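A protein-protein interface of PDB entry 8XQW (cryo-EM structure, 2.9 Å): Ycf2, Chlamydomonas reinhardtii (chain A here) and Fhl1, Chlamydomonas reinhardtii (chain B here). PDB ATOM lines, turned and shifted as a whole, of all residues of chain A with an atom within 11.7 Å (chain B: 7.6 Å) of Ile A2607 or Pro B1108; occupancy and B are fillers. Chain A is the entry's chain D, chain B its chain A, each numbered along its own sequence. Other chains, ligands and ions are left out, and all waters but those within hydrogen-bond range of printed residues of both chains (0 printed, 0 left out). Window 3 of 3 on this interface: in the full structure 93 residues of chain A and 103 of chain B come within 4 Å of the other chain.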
ATOM      1  N   LEU A2598      16.735  -4.540  12.215  1.00  0.00           N
ATOM      2  CA  LEU A2598      17.510  -3.997  13.323  1.00  0.00           C
ATOM      3  C   LEU A2598      16.710  -3.791  14.596  1.00  0.00           C
ATOM      4  O   LEU A2598      17.304  -3.482  15.632  1.00  0.00           O
ATOM      5  CB  LEU A2598      18.122  -2.663  12.929  1.00  0.00           C
ATOM      6  CG  LEU A2598      19.169  -2.714  11.838  1.00  0.00           C
ATOM      7  CD1 LEU A2598      19.854  -1.390  11.786  1.00  0.00           C
ATOM      8  CD2 LEU A2598      20.158  -3.803  12.139  1.00  0.00           C
ATOM      9  N   VAL A2599      15.387  -3.914  14.547  1.00  0.00           N
ATOM     10  CA  VAL A2599      14.584  -3.686  15.739  1.00  0.00           C
ATOM     11  C   VAL A2599      15.002  -4.633  16.847  1.00  0.00           C
ATOM     12  O   VAL A2599      15.069  -4.251  18.021  1.00  0.00           O
ATOM     13  CB  VAL A2599      13.095  -3.838  15.401  1.00  0.00           C
ATOM     14  CG1 VAL A2599      12.296  -4.044  16.650  1.00  0.00           C
ATOM     15  CG2 VAL A2599      12.619  -2.622  14.671  1.00  0.00           C
ATOM     16  N   LYS A2600      15.307  -5.877  16.488  1.00  0.00           N
ATOM     17  CA  LYS A2600      15.681  -6.882  17.474  1.00  0.00           C
ATOM     18  C   LYS A2600      16.842  -6.406  18.331  1.00  0.00           C
ATOM     19  O   LYS A2600      16.734  -6.324  19.557  1.00  0.00           O
ATOM     20  CB  LYS A2600      16.033  -8.181  16.758  1.00  0.00           C
ATOM     21  CG  LYS A2600      14.921  -8.711  15.879  1.00  0.00           C
ATOM     22  CD  LYS A2600      13.876  -9.413  16.717  1.00  0.00           C
ATOM     23  CE  LYS A2600      14.511 -10.519  17.540  1.00  0.00           C
ATOM     24  NZ  LYS A2600      14.212 -10.394  18.987  1.00  0.00           N
ATOM     25  N   SER A2601      17.956  -6.051  17.697  1.00  0.00           N
ATOM     26  CA  SER A2601      19.125  -5.618  18.445  1.00  0.00           C
ATOM     27  C   SER A2601      18.965  -4.233  19.047  1.00  0.00           C
ATOM     28  O   SER A2601      19.562  -3.959  20.090  1.00  0.00           O
ATOM     29  CB  SER A2601      20.352  -5.654  17.547  1.00  0.00           C
ATOM     30  OG  SER A2601      19.992  -5.387  16.210  1.00  0.00           O
ATOM     31  N   LEU A2602      18.183  -3.350  18.430  1.00  0.00           N
ATOM     32  CA  LEU A2602      18.021  -2.021  19.007  1.00  0.00           C
ATOM     33  C   LEU A2602      17.174  -2.058  20.270  1.00  0.00           C
ATOM     34  O   LEU A2602      17.313  -1.191  21.134  1.00  0.00           O
ATOM     35  CB  LEU A2602      17.406  -1.069  17.991  1.00  0.00           C
ATOM     36  CG  LEU A2602      18.389  -0.422  17.029  1.00  0.00           C
ATOM     37  CD1 LEU A2602      17.650   0.340  15.962  1.00  0.00           C
ATOM     38  CD2 LEU A2602      19.312   0.489  17.785  1.00  0.00           C
ATOM     39  N   LYS A2603      16.286  -3.043  20.393  1.00  0.00           N
ATOM     40  CA  LYS A2603      15.487  -3.181  21.602  1.00  0.00           C
ATOM     41  C   LYS A2603      16.046  -4.200  22.583  1.00  0.00           C
ATOM     42  O   LYS A2603      15.621  -4.213  23.742  1.00  0.00           O
ATOM     43  CB  LYS A2603      14.046  -3.566  21.255  1.00  0.00           C
ATOM     44  CG  LYS A2603      13.264  -2.470  20.563  1.00  0.00           C
ATOM     45  CD  LYS A2603      11.949  -2.190  21.265  1.00  0.00           C
ATOM     46  CE  LYS A2603      12.158  -1.295  22.469  1.00  0.00           C
ATOM     47  NZ  LYS A2603      10.970  -1.275  23.359  1.00  0.00           N
ATOM     48  N   GLN A2604      16.979  -5.048  22.157  1.00  0.00           N
ATOM     49  CA  GLN A2604      17.563  -6.029  23.063  1.00  0.00           C
ATOM     50  C   GLN A2604      18.760  -5.468  23.818  1.00  0.00           C
ATOM     51  O   GLN A2604      18.798  -5.516  25.052  1.00  0.00           O
ATOM     52  CB  GLN A2604      17.974  -7.283  22.287  1.00  0.00           C
ATOM     53  CG  GLN A2604      18.937  -8.181  23.029  1.00  0.00           C
ATOM     54  CD  GLN A2604      18.290  -8.866  24.214  1.00  0.00           C
ATOM     55  OE1 GLN A2604      17.194  -9.415  24.104  1.00  0.00           O
ATOM     56  NE2 GLN A2604      18.967  -8.837  25.358  1.00  0.00           N
ATOM     57  N   ALA A2605      19.736  -4.919  23.093  1.00  0.00           N
ATOM     58  CA  ALA A2605      20.947  -4.405  23.722  1.00  0.00           C
ATOM     59  C   ALA A2605      20.662  -3.278  24.708  1.00  0.00           C
ATOM     60  O   ALA A2605      21.587  -2.802  25.373  1.00  0.00           O
ATOM     61  CB  ALA A2605      21.933  -3.931  22.654  1.00  0.00           C
ATOM     62  N   SER A2606      19.411  -2.828  24.805  1.00  0.00           N
ATOM     63  CA  SER A2606      19.003  -1.860  25.815  1.00  0.00           C
ATOM     64  C   SER A2606      17.973  -2.451  26.772  1.00  0.00           C
ATOM     65  O   SER A2606      18.064  -2.251  27.986  1.00  0.00           O
ATOM     66  CB  SER A2606      18.445  -0.599  25.146  1.00  0.00           C
ATOM     67  OG  SER A2606      19.322  -0.113  24.145  1.00  0.00           O
ATOM     68  N   ILE A2607      16.994  -3.176  26.243  1.00  0.00           N
ATOM     69  CA  ILE A2607      15.952  -3.779  27.063  1.00  0.00           C
ATOM     70  C   ILE A2607      16.005  -5.298  26.959  1.00  0.00           C
ATOM     71  O   ILE A2607      15.590  -5.880  25.956  1.00  0.00           O
ATOM     72  CB  ILE A2607      14.563  -3.257  26.664  1.00  0.00           C
ATOM     73  CG1 ILE A2607      14.505  -1.739  26.815  1.00  0.00           C
ATOM     74  CG2 ILE A2607      13.485  -3.912  27.507  1.00  0.00           C
ATOM     75  CD1 ILE A2607      14.616  -1.277  28.243  1.00  0.00           C
ATOM     76  N   PRO A2625       4.123   2.372  19.954  1.00  0.00           N
ATOM     77  CA  PRO A2625       4.591   0.983  19.962  1.00  0.00           C
ATOM     78  C   PRO A2625       5.900   0.784  20.695  1.00  0.00           C
ATOM     79  O   PRO A2625       6.200  -0.342  21.102  1.00  0.00           O
ATOM     80  CB  PRO A2625       4.725   0.658  18.471  1.00  0.00           C
ATOM     81  CG  PRO A2625       3.761   1.538  17.827  1.00  0.00           C
ATOM     82  CD  PRO A2625       3.795   2.818  18.595  1.00  0.00           C
ATOM     83  N   LEU A2626       6.703   1.829  20.875  1.00  0.00           N
ATOM     84  CA  LEU A2626       7.893   1.667  21.694  1.00  0.00           C
ATOM     85  C   LEU A2626       7.599   1.825  23.174  1.00  0.00           C
ATOM     86  O   LEU A2626       8.532   1.825  23.977  1.00  0.00           O
ATOM     87  CB  LEU A2626       8.979   2.653  21.274  1.00  0.00           C
ATOM     88  CG  LEU A2626       8.650   4.129  21.103  1.00  0.00           C
ATOM     89  CD1 LEU A2626       8.761   4.866  22.405  1.00  0.00           C
ATOM     90  CD2 LEU A2626       9.613   4.707  20.125  1.00  0.00           C
ATOM     91  N   GLY A2627       6.329   1.971  23.552  1.00  0.00           N
ATOM     92  CA  GLY A2627       5.984   2.063  24.956  1.00  0.00           C
ATOM     93  C   GLY A2627       5.689   0.737  25.612  1.00  0.00           C
ATOM     94  O   GLY A2627       5.801   0.629  26.836  1.00  0.00           O
ATOM     95  N   GLN A2628       5.309  -0.270  24.831  1.00  0.00           N
ATOM     96  CA  GLN A2628       5.050  -1.592  25.382  1.00  0.00           C
ATOM     97  C   GLN A2628       6.340  -2.203  25.906  1.00  0.00           C
ATOM     98  O   GLN A2628       7.343  -2.271  25.190  1.00  0.00           O
ATOM     99  CB  GLN A2628       4.429  -2.492  24.322  1.00  0.00           C
ATOM    100  CG  GLN A2628       2.920  -2.436  24.280  1.00  0.00           C
ATOM    101  CD  GLN A2628       2.404  -1.264  23.482  1.00  0.00           C
ATOM    102  OE1 GLN A2628       2.796  -0.122  23.711  1.00  0.00           O
ATOM    103  NE2 GLN A2628       1.520  -1.540  22.534  1.00  0.00           N
ATOM    104  N   THR A2629       6.312  -2.647  27.157  1.00  0.00           N
ATOM    105  CA  THR A2629       7.497  -3.103  27.872  1.00  0.00           C
ATOM    106  C   THR A2629       7.377  -4.570  28.267  1.00  0.00           C
ATOM    107  O   THR A2629       7.981  -5.025  29.239  1.00  0.00           O
ATOM    108  CB  THR A2629       7.748  -2.233  29.099  1.00  0.00           C
ATOM    109  OG1 THR A2629       9.017  -2.565  29.672  1.00  0.00           O
ATOM    110  CG2 THR A2629       6.642  -2.413  30.136  1.00  0.00           C
ATOM    111  N   HIS A2630       6.407  -5.244  27.649  1.00  0.00           N
ATOM    112  CA  HIS A2630       6.142  -6.660  28.001  1.00  0.00           C
ATOM    113  C   HIS A2630       6.254  -7.467  26.715  1.00  0.00           C
ATOM    114  O   HIS A2630       7.235  -7.212  25.998  1.00  0.00           O
ATOM    115  CB  HIS A2630       4.747  -6.794  28.606  1.00  0.00           C
ATOM    116  CG  HIS A2630       3.825  -5.706  28.172  1.00  0.00           C
ATOM    117  ND1 HIS A2630       2.984  -5.844  27.089  1.00  0.00           N
ATOM    118  CD2 HIS A2630       3.609  -4.474  28.654  1.00  0.00           C
ATOM    119  CE1 HIS A2630       2.287  -4.728  26.933  1.00  0.00           C
ATOM    120  NE2 HIS A2630       2.654  -3.883  27.870  1.00  0.00           N
ATOM    121  N   LEU A2631       5.300  -8.362  26.444  1.00  0.00           N
ATOM    122  CA  LEU A2631       5.277  -9.145  25.180  1.00  0.00           C
ATOM    123  C   LEU A2631       6.648  -9.768  24.868  1.00  0.00           C
ATOM    124  O   LEU A2631       7.473  -9.091  24.226  1.00  0.00           O
ATOM    125  CB  LEU A2631       4.823  -8.204  24.070  1.00  0.00           C
ATOM    126  CG  LEU A2631       3.375  -7.716  24.139  1.00  0.00           C
ATOM    127  CD1 LEU A2631       3.176  -6.595  23.135  1.00  0.00           C
ATOM    128  CD2 LEU A2631       2.436  -8.871  23.846  1.00  0.00           C
ATOM    129  N   LEU A2632       6.854 -11.034  25.231  1.00  0.00           N
ATOM    130  CA  LEU A2632       8.122 -11.746  24.926  1.00  0.00           C
ATOM    131  C   LEU A2632       8.856 -11.118  23.736  1.00  0.00           C
ATOM    132  O   LEU A2632       8.302 -11.133  22.624  1.00  0.00           O
ATOM    133  CB  LEU A2632       7.751 -13.194  24.633  1.00  0.00           C
ATOM    134  CG  LEU A2632       8.098 -14.212  25.722  1.00  0.00           C
ATOM    135  CD1 LEU A2632       9.231 -13.716  26.601  1.00  0.00           C
ATOM    136  CD2 LEU A2632       6.872 -14.534  26.556  1.00  0.00           C
ATOM    137  N   PRO A2633      10.107 -10.652  23.900  1.00  0.00           N
ATOM    138  CA  PRO A2633      10.830  -9.965  22.830  1.00  0.00           C
ATOM    139  C   PRO A2633      10.728 -10.375  21.356  1.00  0.00           C
ATOM    140  O   PRO A2633      11.261  -9.628  20.524  1.00  0.00           O
ATOM    141  CB  PRO A2633      12.257 -10.194  23.333  1.00  0.00           C
ATOM    142  CG  PRO A2633      12.143 -10.016  24.820  1.00  0.00           C
ATOM    143  CD  PRO A2633      10.855 -10.746  25.138  1.00  0.00           C
ATOM    144  N   LYS A2634      10.117 -11.511  21.032  1.00  0.00           N
ATOM    145  CA  LYS A2634       9.938 -11.877  19.607  1.00  0.00           C
ATOM    146  C   LYS A2634       8.597 -11.331  19.133  1.00  0.00           C
ATOM    147  O   LYS A2634       8.529 -10.734  18.048  1.00  0.00           O
ATOM    148  CB  LYS A2634       9.902 -13.390  19.386  1.00  0.00           C
ATOM    149  CG  LYS A2634      10.443 -13.854  18.044  1.00  0.00           C
ATOM    150  CD  LYS A2634       9.446 -14.687  17.250  1.00  0.00           C
ATOM    151  CE  LYS A2634      10.090 -15.872  16.601  1.00  0.00           C
ATOM    152  NZ  LYS A2634       9.128 -16.938  16.306  1.00  0.00           N
ATOM    153  N   ALA A2635       7.566 -11.553  19.932  1.00  0.00           N
ATOM    154  CA  ALA A2635       6.274 -11.008  19.543  1.00  0.00           C
ATOM    155  C   ALA A2635       6.197  -9.503  19.708  1.00  0.00           C
ATOM    156  O   ALA A2635       5.176  -8.908  19.355  1.00  0.00           O
ATOM    157  CB  ALA A2635       5.152 -11.657  20.354  1.00  0.00           C
ATOM    158  N   LEU A2636       7.236  -8.883  20.254  1.00  0.00           N
ATOM    159  CA  LEU A2636       7.302  -7.435  20.337  1.00  0.00           C
ATOM    160  C   LEU A2636       7.824  -6.808  19.059  1.00  0.00           C
ATOM    161  O   LEU A2636       7.495  -5.658  18.767  1.00  0.00           O
ATOM    162  CB  LEU A2636       8.188  -7.032  21.511  1.00  0.00           C
ATOM    163  CG  LEU A2636       8.595  -5.571  21.643  1.00  0.00           C
ATOM    164  CD1 LEU A2636       7.397  -4.744  22.026  1.00  0.00           C
ATOM    165  CD2 LEU A2636       9.689  -5.430  22.674  1.00  0.00           C
ATOM    166  N   SER A2637       8.606  -7.543  18.280  1.00  0.00           N
ATOM    167  CA  SER A2637       9.227  -6.994  17.087  1.00  0.00           C
ATOM    168  C   SER A2637       8.281  -6.875  15.900  1.00  0.00           C
ATOM    169  O   SER A2637       8.744  -6.557  14.802  1.00  0.00           O
ATOM    170  CB  SER A2637      10.418  -7.854  16.691  1.00  0.00           C
ATOM    171  OG  SER A2637       9.976  -9.020  16.028  1.00  0.00           O
ATOM    172  N   ALA B1101      17.439  11.079  32.426  1.00  0.00           N
ATOM    173  CA  ALA B1101      18.609  10.225  32.544  1.00  0.00           C
ATOM    174  C   ALA B1101      18.369   8.850  31.952  1.00  0.00           C
ATOM    175  O   ALA B1101      19.302   8.244  31.419  1.00  0.00           O
ATOM    176  CB  ALA B1101      19.026  10.092  34.008  1.00  0.00           C
ATOM    177  N   ALA B1102      17.132   8.358  32.013  1.00  0.00           N
ATOM    178  CA  ALA B1102      16.835   7.050  31.438  1.00  0.00           C
ATOM    179  C   ALA B1102      16.821   7.082  29.915  1.00  0.00           C
ATOM    180  O   ALA B1102      16.532   6.064  29.282  1.00  0.00           O
ATOM    181  CB  ALA B1102      15.498   6.535  31.965  1.00  0.00           C
ATOM    182  N   MET B1103      17.107   8.234  29.309  1.00  0.00           N
ATOM    183  CA  MET B1103      17.228   8.347  27.860  1.00  0.00           C
ATOM    184  C   MET B1103      18.548   8.972  27.434  1.00  0.00           C
ATOM    185  O   MET B1103      18.742   9.228  26.247  1.00  0.00           O
ATOM    186  CB  MET B1103      16.064   9.153  27.281  1.00  0.00           C
ATOM    187  CG  MET B1103      14.695   8.632  27.660  1.00  0.00           C
ATOM    188  SD  MET B1103      13.362   9.314  26.660  1.00  0.00           S
ATOM    189  CE  MET B1103      13.392   8.223  25.243  1.00  0.00           C
ATOM    190  N   SER B1104      19.448   9.234  28.371  1.00  0.00           N
ATOM    191  CA  SER B1104      20.790   9.661  28.029  1.00  0.00           C
ATOM    192  C   SER B1104      21.588   8.465  27.513  1.00  0.00           C
ATOM    193  O   SER B1104      21.169   7.319  27.687  1.00  0.00           O
ATOM    194  CB  SER B1104      21.452  10.285  29.251  1.00  0.00           C
ATOM    195  OG  SER B1104      20.982   9.674  30.434  1.00  0.00           O
ATOM    196  N   PRO B1105      22.734   8.698  26.862  1.00  0.00           N
ATOM    197  CA  PRO B1105      23.458   7.570  26.254  1.00  0.00           C
ATOM    198  C   PRO B1105      23.753   6.446  27.224  1.00  0.00           C
ATOM    199  O   PRO B1105      23.796   5.279  26.819  1.00  0.00           O
ATOM    200  CB  PRO B1105      24.746   8.220  25.741  1.00  0.00           C
ATOM    201  CG  PRO B1105      24.390   9.618  25.534  1.00  0.00           C
ATOM    202  CD  PRO B1105      23.445   9.962  26.632  1.00  0.00           C
ATOM    203  N   SER B1106      23.947   6.762  28.497  1.00  0.00           N
ATOM    204  CA  SER B1106      24.107   5.745  29.530  1.00  0.00           C
ATOM    205  C   SER B1106      22.763   5.384  30.148  1.00  0.00           C
ATOM    206  O   SER B1106      22.586   5.409  31.363  1.00  0.00           O
ATOM    207  CB  SER B1106      25.085   6.241  30.583  1.00  0.00           C
ATOM    208  OG  SER B1106      26.320   6.583  29.984  1.00  0.00           O
ATOM    209  N   GLY B1107      21.800   5.047  29.297  1.00  0.00           N
ATOM    210  CA  GLY B1107      20.472   4.721  29.751  1.00  0.00           C
ATOM    211  C   GLY B1107      19.920   3.484  29.078  1.00  0.00           C
ATOM    212  O   GLY B1107      20.425   3.026  28.051  1.00  0.00           O
ATOM    213  N   PRO B1108      18.880   2.916  29.651  1.00  0.00           N
ATOM    214  CA  PRO B1108      18.281   1.716  29.066  1.00  0.00           C
ATOM    215  C   PRO B1108      17.316   1.987  27.922  1.00  0.00           C
ATOM    216  O   PRO B1108      16.801   1.041  27.322  1.00  0.00           O
ATOM    217  CB  PRO B1108      17.557   1.081  30.255  1.00  0.00           C
ATOM    218  CG  PRO B1108      17.272   2.206  31.159  1.00  0.00           C
ATOM    219  CD  PRO B1108      18.417   3.151  31.025  1.00  0.00           C
ATOM    220  N   LEU B1109      17.038   3.248  27.609  1.00  0.00           N
ATOM    221  CA  LEU B1109      16.081   3.574  26.562  1.00  0.00           C
ATOM    222  C   LEU B1109      16.686   4.357  25.415  1.00  0.00           C
ATOM    223  O   LEU B1109      15.942   4.893  24.594  1.00  0.00           O
ATOM    224  CB  LEU B1109      14.906   4.359  27.134  1.00  0.00           C
ATOM    225  CG  LEU B1109      14.122   3.712  28.262  1.00  0.00           C
ATOM    226  CD1 LEU B1109      12.912   4.552  28.560  1.00  0.00           C
ATOM    227  CD2 LEU B1109      13.718   2.315  27.877  1.00  0.00           C
ATOM    228  N   TYR B1110      18.008   4.449  25.336  1.00  0.00           N
ATOM    229  CA  TYR B1110      18.622   5.242  24.280  1.00  0.00           C
ATOM    230  C   TYR B1110      18.276   4.692  22.905  1.00  0.00           C
ATOM    231  O   TYR B1110      18.043   5.457  21.965  1.00  0.00           O
ATOM    232  CB  TYR B1110      20.130   5.281  24.475  1.00  0.00           C
ATOM    233  CG  TYR B1110      20.822   6.361  23.708  1.00  0.00           C
ATOM    234  CD1 TYR B1110      20.329   7.644  23.692  1.00  0.00           C
ATOM    235  CD2 TYR B1110      21.978   6.098  23.005  1.00  0.00           C
ATOM    236  CE1 TYR B1110      20.964   8.634  22.992  1.00  0.00           C
ATOM    237  CE2 TYR B1110      22.622   7.081  22.305  1.00  0.00           C
ATOM    238  CZ  TYR B1110      22.110   8.349  22.301  1.00  0.00           C
ATOM    239  OH  TYR B1110      22.748   9.340  21.601  1.00  0.00           O
ATOM    240  N   GLY B1111      18.219   3.371  22.772  1.00  0.00           N
ATOM    241  CA  GLY B1111      17.976   2.776  21.471  1.00  0.00           C
ATOM    242  C   GLY B1111      16.669   3.202  20.839  1.00  0.00           C
ATOM    243  O   GLY B1111      16.577   3.312  19.618  1.00  0.00           O
ATOM    244  N   ASN B1112      15.644   3.451  21.653  1.00  0.00           N
ATOM    245  CA  ASN B1112      14.363   3.892  21.121  1.00  0.00           C
ATOM    246  C   ASN B1112      14.454   5.204  20.366  1.00  0.00           C
ATOM    247  O   ASN B1112      13.531   5.531  19.622  1.00  0.00           O
ATOM    248  CB  ASN B1112      13.349   4.036  22.239  1.00  0.00           C
ATOM    249  CG  ASN B1112      13.101   2.746  22.952  1.00  0.00           C
ATOM    250  OD1 ASN B1112      13.781   1.755  22.707  1.00  0.00           O
ATOM    251  ND2 ASN B1112      12.121   2.740  23.839  1.00  0.00           N
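Among the printed residues, pairs that only touch across the chains: Lys A2603 with Asn B1112 (3.5 Å), Ser A2606 with Pro B1108 (3.2 Å), Ser A2606 with Gly B1111 (3.9 Å), Ile A2607 with Pro B1108 (3.3 Å), Ile A2607 with Leu B1109 (3.7 Å) and Leu A2626 with Asn B1112 (3.7 Å).
No residue of chain A comes within 4 Å of Gly B1107.
Leu B1109 touches just one residue of chain A: Ile A2607 (3.7 Å).
Of the printed residues of chain A, Asn B1112 touches Lys A2603 and Leu A2626.
Printed residues of chain A within 4 Å of Gly B1111: Ser A2606 (3.9 Å).
Printed residues of chain B within 4 Å of Leu A2626: Asn B1112.
Of the printed residues of chain B, Ser A2606 touches Pro B1108 (3.2 Å) and Gly B1111 (3.9 Å).
Gln A2628 touches none of the printed residues of chain B.
Ser A2637 touches none of the printed residues of chain B.
The nearest residue of chain B that does not touch Ile A2607 is Asn B1112 (5.4 Å).
The nearest residue of chain A that does not touch Pro B1108 is Ala A2605 (6.4 Å).
The nearest printed residue of chain B that does not touch Ser A2606 is Leu B1109 (4.8 Å).
Hydrophobic or aromatic side chains of chain A within 4 Å of the printed part of chain B: Ile A2607.
Printed residues of chain B that touch a printed residue of chain A: Pro B1108, Leu B1109, Gly B1111 and Asn B1112.
Hydrophobic or aromatic side chains of chain B within 4 Å of the printed part of chain A: Leu B1109.
Along chain B the printed residues that touch a printed residue of chain A span positions 1108 to 1112.
Among the printed residues, no Asp or Glu carboxylate lies within 4 Å of a Lys or Arg side-chain nitrogen of the other chain.
O of Ala B1102 sits close to N of Leu B1109, at 3.3 Å.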
